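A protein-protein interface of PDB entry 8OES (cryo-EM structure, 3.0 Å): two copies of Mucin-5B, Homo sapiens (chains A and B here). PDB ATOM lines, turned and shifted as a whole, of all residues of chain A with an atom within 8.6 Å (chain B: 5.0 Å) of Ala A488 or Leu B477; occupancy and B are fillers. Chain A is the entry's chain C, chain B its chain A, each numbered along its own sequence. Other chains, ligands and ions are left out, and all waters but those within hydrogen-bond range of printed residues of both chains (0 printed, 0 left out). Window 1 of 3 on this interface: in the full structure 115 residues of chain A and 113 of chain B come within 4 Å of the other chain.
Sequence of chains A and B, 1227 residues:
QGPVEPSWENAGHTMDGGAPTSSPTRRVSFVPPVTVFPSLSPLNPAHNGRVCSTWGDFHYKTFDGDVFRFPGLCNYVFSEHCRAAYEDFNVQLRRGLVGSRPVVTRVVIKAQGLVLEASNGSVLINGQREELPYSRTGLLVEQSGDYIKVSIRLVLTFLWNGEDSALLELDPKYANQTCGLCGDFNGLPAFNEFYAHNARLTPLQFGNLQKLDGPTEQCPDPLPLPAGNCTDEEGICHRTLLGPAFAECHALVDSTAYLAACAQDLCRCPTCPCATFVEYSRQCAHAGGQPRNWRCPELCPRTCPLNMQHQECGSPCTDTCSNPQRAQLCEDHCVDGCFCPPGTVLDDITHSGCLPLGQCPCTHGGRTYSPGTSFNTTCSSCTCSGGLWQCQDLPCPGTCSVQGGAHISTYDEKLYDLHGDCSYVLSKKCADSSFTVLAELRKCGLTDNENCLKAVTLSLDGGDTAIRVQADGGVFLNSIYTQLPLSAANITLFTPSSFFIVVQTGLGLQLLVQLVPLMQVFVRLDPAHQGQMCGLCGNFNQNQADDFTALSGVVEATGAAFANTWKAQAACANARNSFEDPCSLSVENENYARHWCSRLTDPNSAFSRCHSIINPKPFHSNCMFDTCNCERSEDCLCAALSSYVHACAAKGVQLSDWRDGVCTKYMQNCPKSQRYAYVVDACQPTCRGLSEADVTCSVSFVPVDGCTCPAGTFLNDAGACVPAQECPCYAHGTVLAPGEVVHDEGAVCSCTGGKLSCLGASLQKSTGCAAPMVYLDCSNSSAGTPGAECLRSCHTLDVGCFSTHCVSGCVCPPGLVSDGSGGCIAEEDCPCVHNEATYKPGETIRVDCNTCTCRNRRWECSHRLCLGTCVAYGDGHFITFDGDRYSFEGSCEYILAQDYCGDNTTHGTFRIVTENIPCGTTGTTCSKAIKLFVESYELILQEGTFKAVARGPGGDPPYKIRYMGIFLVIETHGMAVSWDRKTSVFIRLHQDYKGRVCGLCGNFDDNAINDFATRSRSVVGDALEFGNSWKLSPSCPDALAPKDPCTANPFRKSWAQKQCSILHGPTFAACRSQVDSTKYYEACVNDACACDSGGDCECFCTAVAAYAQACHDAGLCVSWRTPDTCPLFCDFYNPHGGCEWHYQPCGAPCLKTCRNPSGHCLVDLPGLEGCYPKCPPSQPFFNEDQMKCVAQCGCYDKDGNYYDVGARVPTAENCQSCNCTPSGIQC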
ATOM      1  N   LEU A 460      -7.276 -40.245 -18.699  1.00  0.00           N
ATOM      2  CA  LEU A 460      -6.688 -39.103 -19.376  1.00  0.00           C
ATOM      3  C   LEU A 460      -5.696 -38.419 -18.448  1.00  0.00           C
ATOM      4  O   LEU A 460      -5.860 -38.426 -17.222  1.00  0.00           O
ATOM      5  CB  LEU A 460      -7.790 -38.138 -19.821  1.00  0.00           C
ATOM      6  CG  LEU A 460      -7.464 -36.853 -20.567  1.00  0.00           C
ATOM      7  CD1 LEU A 460      -8.474 -36.653 -21.667  1.00  0.00           C
ATOM      8  CD2 LEU A 460      -7.506 -35.686 -19.613  1.00  0.00           C
ATOM      9  N   THR A 465      -7.701 -37.623 -15.045  1.00  0.00           N
ATOM     10  CA  THR A 465      -9.111 -37.442 -15.357  1.00  0.00           C
ATOM     11  C   THR A 465      -9.670 -38.761 -15.869  1.00  0.00           C
ATOM     12  O   THR A 465      -8.941 -39.557 -16.463  1.00  0.00           O
ATOM     13  CB  THR A 465      -9.304 -36.326 -16.388  1.00  0.00           C
ATOM     14  OG1 THR A 465      -8.910 -35.079 -15.806  1.00  0.00           O
ATOM     15  CG2 THR A 465     -10.752 -36.212 -16.807  1.00  0.00           C
ATOM     16  N   ILE A 467     -13.392 -40.031 -17.640  1.00  0.00           N
ATOM     17  CA  ILE A 467     -14.765 -39.850 -18.091  1.00  0.00           C
ATOM     18  C   ILE A 467     -15.341 -41.232 -18.344  1.00  0.00           C
ATOM     19  O   ILE A 467     -14.892 -41.942 -19.245  1.00  0.00           O
ATOM     20  CB  ILE A 467     -14.833 -38.983 -19.351  1.00  0.00           C
ATOM     21  CG1 ILE A 467     -14.117 -37.658 -19.122  1.00  0.00           C
ATOM     22  CG2 ILE A 467     -16.261 -38.743 -19.742  1.00  0.00           C
ATOM     23  CD1 ILE A 467     -13.610 -37.036 -20.386  1.00  0.00           C
ATOM     24  N   LEU A 477     -17.968 -37.927 -14.535  1.00  0.00           N
ATOM     25  CA  LEU A 477     -16.735 -37.159 -14.651  1.00  0.00           C
ATOM     26  C   LEU A 477     -15.974 -37.304 -13.340  1.00  0.00           C
ATOM     27  O   LEU A 477     -16.447 -36.853 -12.293  1.00  0.00           O
ATOM     28  CB  LEU A 477     -17.028 -35.696 -14.965  1.00  0.00           C
ATOM     29  CG  LEU A 477     -15.831 -34.833 -15.359  1.00  0.00           C
ATOM     30  CD1 LEU A 477     -15.496 -35.001 -16.825  1.00  0.00           C
ATOM     31  CD2 LEU A 477     -16.097 -33.380 -15.039  1.00  0.00           C
ATOM     32  N   THR A 482     -22.287 -36.377 -13.981  1.00  0.00           N
ATOM     33  CA  THR A 482     -22.220 -35.138 -14.742  1.00  0.00           C
ATOM     34  C   THR A 482     -23.195 -35.236 -15.898  1.00  0.00           C
ATOM     35  O   THR A 482     -23.017 -36.073 -16.784  1.00  0.00           O
ATOM     36  CB  THR A 482     -20.812 -34.888 -15.266  1.00  0.00           C
ATOM     37  OG1 THR A 482     -19.970 -34.475 -14.185  1.00  0.00           O
ATOM     38  CG2 THR A 482     -20.836 -33.814 -16.327  1.00  0.00           C
ATOM     39  N   PRO A 485     -24.855 -31.371 -21.873  1.00  0.00           N
ATOM     40  CA  PRO A 485     -23.428 -31.341 -22.231  1.00  0.00           C
ATOM     41  C   PRO A 485     -22.488 -30.859 -21.135  1.00  0.00           C
ATOM     42  O   PRO A 485     -22.912 -30.359 -20.104  1.00  0.00           O
ATOM     43  CB  PRO A 485     -23.407 -30.374 -23.417  1.00  0.00           C
ATOM     44  CG  PRO A 485     -24.487 -29.408 -23.103  1.00  0.00           C
ATOM     45  CD  PRO A 485     -25.569 -30.210 -22.429  1.00  0.00           C
ATOM     46  N   LEU A 486     -21.184 -31.021 -21.345  1.00  0.00           N
ATOM     47  CA  LEU A 486     -20.166 -30.454 -20.474  1.00  0.00           C
ATOM     48  C   LEU A 486     -18.940 -30.101 -21.299  1.00  0.00           C
ATOM     49  O   LEU A 486     -18.456 -30.919 -22.082  1.00  0.00           O
ATOM     50  CB  LEU A 486     -19.764 -31.412 -19.356  1.00  0.00           C
ATOM     51  CG  LEU A 486     -18.542 -30.922 -18.581  1.00  0.00           C
ATOM     52  CD1 LEU A 486     -18.805 -30.938 -17.093  1.00  0.00           C
ATOM     53  CD2 LEU A 486     -17.318 -31.756 -18.918  1.00  0.00           C
ATOM     54  N   SER A 487     -18.412 -28.896 -21.095  1.00  0.00           N
ATOM     55  CA  SER A 487     -17.287 -28.405 -21.889  1.00  0.00           C
ATOM     56  C   SER A 487     -16.227 -27.845 -20.952  1.00  0.00           C
ATOM     57  O   SER A 487     -16.392 -26.750 -20.415  1.00  0.00           O
ATOM     58  CB  SER A 487     -17.746 -27.343 -22.888  1.00  0.00           C
ATOM     59  OG  SER A 487     -16.677 -26.930 -23.717  1.00  0.00           O
ATOM     60  N   ALA A 488     -15.135 -28.583 -20.774  1.00  0.00           N
ATOM     61  CA  ALA A 488     -14.069 -28.140 -19.887  1.00  0.00           C
ATOM     62  C   ALA A 488     -12.795 -28.909 -20.189  1.00  0.00           C
ATOM     63  O   ALA A 488     -12.849 -30.089 -20.535  1.00  0.00           O
ATOM     64  CB  ALA A 488     -14.449 -28.332 -18.419  1.00  0.00           C
ATOM     65  N   ALA A 489     -11.655 -28.236 -20.029  1.00  0.00           N
ATOM     66  CA  ALA A 489     -10.344 -28.818 -20.319  1.00  0.00           C
ATOM     67  C   ALA A 489     -10.274 -29.317 -21.760  1.00  0.00           C
ATOM     68  O   ALA A 489      -9.644 -30.335 -22.056  1.00  0.00           O
ATOM     69  CB  ALA A 489     -10.000 -29.936 -19.333  1.00  0.00           C
ATOM     70  N   ASN A 490     -10.935 -28.588 -22.659  1.00  0.00           N
ATOM     71  CA  ASN A 490     -11.076 -28.887 -24.081  1.00  0.00           C
ATOM     72  C   ASN A 490     -11.938 -30.112 -24.349  1.00  0.00           C
ATOM     73  O   ASN A 490     -12.154 -30.459 -25.514  1.00  0.00           O
ATOM     74  CB  ASN A 490      -9.720 -29.064 -24.778  1.00  0.00           C
ATOM     75  CG  ASN A 490      -8.775 -27.903 -24.533  1.00  0.00           C
ATOM     76  OD1 ASN A 490      -8.832 -26.883 -25.217  1.00  0.00           O
ATOM     77  ND2 ASN A 490      -7.892 -28.062 -23.557  1.00  0.00           N
ATOM     78  N   ILE A 491     -12.459 -30.764 -23.314  1.00  0.00           N
ATOM     79  CA  ILE A 491     -13.288 -31.954 -23.463  1.00  0.00           C
ATOM     80  C   ILE A 491     -14.746 -31.529 -23.557  1.00  0.00           C
ATOM     81  O   ILE A 491     -15.228 -30.753 -22.724  1.00  0.00           O
ATOM     82  CB  ILE A 491     -13.080 -32.928 -22.295  1.00  0.00           C
ATOM     83  CG1 ILE A 491     -11.640 -32.862 -21.797  1.00  0.00           C
ATOM     84  CG2 ILE A 491     -13.407 -34.330 -22.728  1.00  0.00           C
ATOM     85  CD1 ILE A 491     -10.643 -33.472 -22.742  1.00  0.00           C
ATOM     86  N   THR A 492     -15.445 -32.044 -24.565  1.00  0.00           N
ATOM     87  CA  THR A 492     -16.832 -31.697 -24.848  1.00  0.00           C
ATOM     88  C   THR A 492     -17.666 -32.966 -24.869  1.00  0.00           C
ATOM     89  O   THR A 492     -17.416 -33.861 -25.678  1.00  0.00           O
ATOM     90  CB  THR A 492     -16.950 -30.977 -26.188  1.00  0.00           C
ATOM     91  OG1 THR A 492     -15.898 -30.016 -26.313  1.00  0.00           O
ATOM     92  CG2 THR A 492     -18.282 -30.280 -26.297  1.00  0.00           C
ATOM     93  N   LEU A 493     -18.664 -33.036 -24.000  1.00  0.00           N
ATOM     94  CA  LEU A 493     -19.558 -34.181 -23.910  1.00  0.00           C
ATOM     95  C   LEU A 493     -20.957 -33.716 -24.271  1.00  0.00           C
ATOM     96  O   LEU A 493     -21.471 -32.775 -23.660  1.00  0.00           O
ATOM     97  CB  LEU A 493     -19.552 -34.771 -22.502  1.00  0.00           C
ATOM     98  CG  LEU A 493     -18.432 -35.688 -22.034  1.00  0.00           C
ATOM     99  CD1 LEU A 493     -17.090 -34.997 -22.084  1.00  0.00           C
ATOM    100  CD2 LEU A 493     -18.740 -36.104 -20.626  1.00  0.00           C
ATOM    101  N   GLN A 504     -15.707 -35.658 -27.122  1.00  0.00           N
ATOM    102  CA  GLN A 504     -14.705 -35.089 -28.010  1.00  0.00           C
ATOM    103  C   GLN A 504     -13.582 -34.489 -27.182  1.00  0.00           C
ATOM    104  O   GLN A 504     -13.834 -33.679 -26.290  1.00  0.00           O
ATOM    105  CB  GLN A 504     -15.340 -34.020 -28.894  1.00  0.00           C
ATOM    106  CG  GLN A 504     -14.366 -33.033 -29.461  1.00  0.00           C
ATOM    107  CD  GLN A 504     -13.453 -33.656 -30.467  1.00  0.00           C
ATOM    108  OE1 GLN A 504     -13.895 -34.125 -31.511  1.00  0.00           O
ATOM    109  NE2 GLN A 504     -12.166 -33.667 -30.169  1.00  0.00           N
ATOM    110  N   THR A 505     -12.347 -34.878 -27.472  1.00  0.00           N
ATOM    111  CA  THR A 505     -11.204 -34.344 -26.752  1.00  0.00           C
ATOM    112  C   THR A 505     -10.256 -33.658 -27.722  1.00  0.00           C
ATOM    113  O   THR A 505     -10.267 -33.919 -28.924  1.00  0.00           O
ATOM    114  CB  THR A 505     -10.447 -35.433 -25.981  1.00  0.00           C
ATOM    115  OG1 THR A 505      -9.717 -36.254 -26.894  1.00  0.00           O
ATOM    116  CG2 THR A 505     -11.417 -36.297 -25.218  1.00  0.00           C
ATOM    117  N   GLY A 506      -9.443 -32.758 -27.182  1.00  0.00           N
ATOM    118  CA  GLY A 506      -8.432 -32.110 -27.985  1.00  0.00           C
ATOM    119  C   GLY A 506      -7.164 -32.905 -28.162  1.00  0.00           C
ATOM    120  O   GLY A 506      -6.346 -32.552 -29.014  1.00  0.00           O
ATOM    121  N   VAL A 695     -20.257 -23.957 -27.708  1.00  0.00           N
ATOM    122  CA  VAL A 695     -19.062 -24.722 -28.037  1.00  0.00           C
ATOM    123  C   VAL A 695     -19.425 -26.085 -28.601  1.00  0.00           C
ATOM    124  O   VAL A 695     -18.682 -26.631 -29.424  1.00  0.00           O
ATOM    125  CB  VAL A 695     -18.164 -24.841 -26.788  1.00  0.00           C
ATOM    126  CG1 VAL A 695     -17.333 -26.108 -26.809  1.00  0.00           C
ATOM    127  CG2 VAL A 695     -17.254 -23.629 -26.676  1.00  0.00           C
ATOM    128  N   THR B 465     -11.728 -20.242 -19.230  1.00  0.00           N
ATOM    129  CA  THR B 465     -12.773 -20.897 -18.456  1.00  0.00           C
ATOM    130  C   THR B 465     -13.539 -19.837 -17.680  1.00  0.00           C
ATOM    131  O   THR B 465     -12.979 -18.800 -17.322  1.00  0.00           O
ATOM    132  CB  THR B 465     -12.177 -21.947 -17.514  1.00  0.00           C
ATOM    133  OG1 THR B 465     -11.602 -23.001 -18.291  1.00  0.00           O
ATOM    134  CG2 THR B 465     -13.239 -22.546 -16.621  1.00  0.00           C
ATOM    135  N   ALA B 466     -14.826 -20.077 -17.450  1.00  0.00           N
ATOM    136  CA  ALA B 466     -15.662 -19.124 -16.729  1.00  0.00           C
ATOM    137  C   ALA B 466     -16.705 -19.895 -15.938  1.00  0.00           C
ATOM    138  O   ALA B 466     -17.616 -20.485 -16.521  1.00  0.00           O
ATOM    139  CB  ALA B 466     -16.323 -18.136 -17.688  1.00  0.00           C
ATOM    140  N   ILE B 467     -16.577 -19.882 -14.620  1.00  0.00           N
ATOM    141  CA  ILE B 467     -17.540 -20.515 -13.729  1.00  0.00           C
ATOM    142  C   ILE B 467     -18.437 -19.417 -13.182  1.00  0.00           C
ATOM    143  O   ILE B 467     -17.979 -18.543 -12.445  1.00  0.00           O
ATOM    144  CB  ILE B 467     -16.844 -21.274 -12.595  1.00  0.00           C
ATOM    145  CG1 ILE B 467     -15.837 -22.267 -13.163  1.00  0.00           C
ATOM    146  CG2 ILE B 467     -17.855 -21.986 -11.747  1.00  0.00           C
ATOM    147  CD1 ILE B 467     -14.728 -22.591 -12.212  1.00  0.00           C
ATOM    148  N   VAL B 475     -25.332 -22.924 -11.500  1.00  0.00           N
ATOM    149  CA  VAL B 475     -23.902 -22.823 -11.755  1.00  0.00           C
ATOM    150  C   VAL B 475     -23.653 -23.123 -13.222  1.00  0.00           C
ATOM    151  O   VAL B 475     -24.039 -24.186 -13.717  1.00  0.00           O
ATOM    152  CB  VAL B 475     -23.103 -23.780 -10.862  1.00  0.00           C
ATOM    153  CG1 VAL B 475     -21.636 -23.521 -11.026  1.00  0.00           C
ATOM    154  CG2 VAL B 475     -23.521 -23.621  -9.422  1.00  0.00           C
ATOM    155  N   PHE B 476     -23.001 -22.199 -13.909  1.00  0.00           N
ATOM    156  CA  PHE B 476     -22.764 -22.291 -15.342  1.00  0.00           C
ATOM    157  C   PHE B 476     -21.276 -22.492 -15.562  1.00  0.00           C
ATOM    158  O   PHE B 476     -20.482 -21.592 -15.287  1.00  0.00           O
ATOM    159  CB  PHE B 476     -23.235 -21.026 -16.053  1.00  0.00           C
ATOM    160  CG  PHE B 476     -24.723 -20.925 -16.214  1.00  0.00           C
ATOM    161  CD1 PHE B 476     -25.571 -21.160 -15.152  1.00  0.00           C
ATOM    162  CD2 PHE B 476     -25.266 -20.566 -17.428  1.00  0.00           C
ATOM    163  CE1 PHE B 476     -26.925 -21.057 -15.305  1.00  0.00           C
ATOM    164  CE2 PHE B 476     -26.619 -20.462 -17.583  1.00  0.00           C
ATOM    165  CZ  PHE B 476     -27.450 -20.707 -16.521  1.00  0.00           C
ATOM    166  N   LEU B 477     -20.896 -23.658 -16.063  1.00  0.00           N
ATOM    167  CA  LEU B 477     -19.518 -23.926 -16.449  1.00  0.00           C
ATOM    168  C   LEU B 477     -19.378 -23.596 -17.929  1.00  0.00           C
ATOM    169  O   LEU B 477     -20.000 -24.245 -18.773  1.00  0.00           O
ATOM    170  CB  LEU B 477     -19.141 -25.377 -16.167  1.00  0.00           C
ATOM    171  CG  LEU B 477     -17.660 -25.730 -16.288  1.00  0.00           C
ATOM    172  CD1 LEU B 477     -16.908 -25.369 -15.025  1.00  0.00           C
ATOM    173  CD2 LEU B 477     -17.491 -27.199 -16.605  1.00  0.00           C
ATOM    174  N   ASN B 478     -18.571 -22.584 -18.237  1.00  0.00           N
ATOM    175  CA  ASN B 478     -18.387 -22.109 -19.605  1.00  0.00           C
ATOM    176  C   ASN B 478     -19.729 -21.837 -20.275  1.00  0.00           C
ATOM    177  O   ASN B 478     -19.985 -22.254 -21.406  1.00  0.00           O
ATOM    178  CB  ASN B 478     -17.558 -23.096 -20.414  1.00  0.00           C
ATOM    179  CG  ASN B 478     -16.293 -23.490 -19.707  1.00  0.00           C
ATOM    180  OD1 ASN B 478     -16.323 -23.905 -18.553  1.00  0.00           O
ATOM    181  ND2 ASN B 478     -15.165 -23.358 -20.391  1.00  0.00           N
ATOM    182  N   SER B 479     -20.596 -21.132 -19.548  1.00  0.00           N
ATOM    183  CA  SER B 479     -21.924 -20.742 -20.025  1.00  0.00           C
ATOM    184  C   SER B 479     -22.786 -21.950 -20.355  1.00  0.00           C
ATOM    185  O   SER B 479     -23.622 -21.900 -21.255  1.00  0.00           O
ATOM    186  CB  SER B 479     -21.835 -19.809 -21.235  1.00  0.00           C
ATOM    187  OG  SER B 479     -21.314 -20.485 -22.366  1.00  0.00           O
ATOM    188  N   ILE B 480     -22.582 -23.045 -19.636  1.00  0.00           N
ATOM    189  CA  ILE B 480     -23.400 -24.241 -19.763  1.00  0.00           C
ATOM    190  C   ILE B 480     -23.804 -24.661 -18.364  1.00  0.00           C
ATOM    191  O   ILE B 480     -22.979 -24.627 -17.448  1.00  0.00           O
ATOM    192  CB  ILE B 480     -22.647 -25.380 -20.473  1.00  0.00           C
ATOM    193  CG1 ILE B 480     -22.409 -25.029 -21.938  1.00  0.00           C
ATOM    194  CG2 ILE B 480     -23.413 -26.677 -20.370  1.00  0.00           C
ATOM    195  CD1 ILE B 480     -21.089 -25.515 -22.467  1.00  0.00           C
ATOM    196  N   TYR B 481     -25.068 -25.035 -18.189  1.00  0.00           N
ATOM    197  CA  TYR B 481     -25.515 -25.497 -16.883  1.00  0.00           C
ATOM    198  C   TYR B 481     -24.707 -26.704 -16.437  1.00  0.00           C
ATOM    199  O   TYR B 481     -24.470 -27.637 -17.207  1.00  0.00           O
ATOM    200  CB  TYR B 481     -26.993 -25.857 -16.910  1.00  0.00           C
ATOM    201  CG  TYR B 481     -27.569 -26.083 -15.537  1.00  0.00           C
ATOM    202  CD1 TYR B 481     -27.825 -25.021 -14.692  1.00  0.00           C
ATOM    203  CD2 TYR B 481     -27.842 -27.361 -15.079  1.00  0.00           C
ATOM    204  CE1 TYR B 481     -28.349 -25.223 -13.437  1.00  0.00           C
ATOM    205  CE2 TYR B 481     -28.366 -27.572 -13.822  1.00  0.00           C
ATOM    206  CZ  TYR B 481     -28.616 -26.498 -13.006  1.00  0.00           C
ATOM    207  OH  TYR B 481     -29.136 -26.693 -11.753  1.00  0.00           O
ATOM    208  N   THR B 482     -24.282 -26.679 -15.178  1.00  0.00           N
ATOM    209  CA  THR B 482     -23.513 -27.766 -14.588  1.00  0.00           C
ATOM    210  C   THR B 482     -23.981 -27.955 -13.158  1.00  0.00           C
ATOM    211  O   THR B 482     -23.806 -27.061 -12.330  1.00  0.00           O
ATOM    212  CB  THR B 482     -22.020 -27.464 -14.615  1.00  0.00           C
ATOM    213  OG1 THR B 482     -21.531 -27.611 -15.951  1.00  0.00           O
ATOM    214  CG2 THR B 482     -21.285 -28.413 -13.699  1.00  0.00           C
ATOM    215  N   LEU B 486     -18.809 -30.850  -9.111  1.00  0.00           N
ATOM    216  CA  LEU B 486     -18.039 -31.065 -10.327  1.00  0.00           C
ATOM    217  C   LEU B 486     -16.559 -30.908 -10.017  1.00  0.00           C
ATOM    218  O   LEU B 486     -16.152 -29.927  -9.395  1.00  0.00           O
ATOM    219  CB  LEU B 486     -18.429 -30.093 -11.437  1.00  0.00           C
ATOM    220  CG  LEU B 486     -17.474 -30.158 -12.629  1.00  0.00           C
ATOM    221  CD1 LEU B 486     -18.236 -30.323 -13.923  1.00  0.00           C
ATOM    222  CD2 LEU B 486     -16.591 -28.924 -12.681  1.00  0.00           C
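OD1 of Asn B478 sits close to O of Ser A487, 3.4 Å away.
N of Asn B478 sits at hydrogen-bond distance from O of Ala B466, 2.9 Å away.
O of Leu A486 lies within hydrogen-bond range of N of Leu A493, 2.9 Å away.
Among the printed residues, merely in contact across the chains: Leu A477 with Leu B486 (3.9 Å), Pro A485 with Ile B480 (3.7 Å), Leu A486 with Leu B477 (3.99 Å), Leu A486 with Leu B486 (3.3 Å), Ser A487 with Leu B477 (3.99 Å), Ser A487 with Ile B480 (3.8 Å) and Ala A488 with Leu B477 (3.7 Å).
Of chain B, only Leu B477 (3.7 Å) comes within 4 Å of Ala A488.
Printed residues of chain A within 4 Å of Leu B477: Leu A486, Ser A487 and Ala A488.
Ile B480 touches just these residues of chain A: Pro A485 (3.7 Å) and Ser A487 (3.8 Å).
Of the printed residues of chain B, Ser A487 touches Leu B477 (3.99 Å), Asn B478 (3.3 Å) and Ile B480 (3.8 Å).
Of the printed residues of chain A, Asn B478 touches Ser A487 (3.3 Å).
Ile A467 touches none of the printed residues of chain B.
The nearest printed residue of chain A that does not touch Leu B477 is Leu A477 (6.5 Å).
Of the 12 printed residues of chain B, 4 touch a printed residue of chain A.
Hydrophobic or aromatic side chains of chain B within 4 Å of the printed part of chain A: Leu B477, Ile B480 and Leu B486.
Printed residues of chain A that touch a printed residue of chain B: Leu A477, Pro A485, Leu A486, Ser A487 and Ala A488.
Among the printed residues, no Asp or Glu carboxylate lies within 4 Å of a Lys or Arg side-chain nitrogen of the other chain.
Leu A477 touches Leu B486, and with the chains exchanged Leu A486 touches Leu B477.
Leu B486 touches its own counterpart, Leu A486.
Positions printed for both chains: 465, 467, 477, 482 and 486.
Of the 8 pairs that touch across the chains among the printed residues, 3 have their exchanged pair printed and touching as well.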
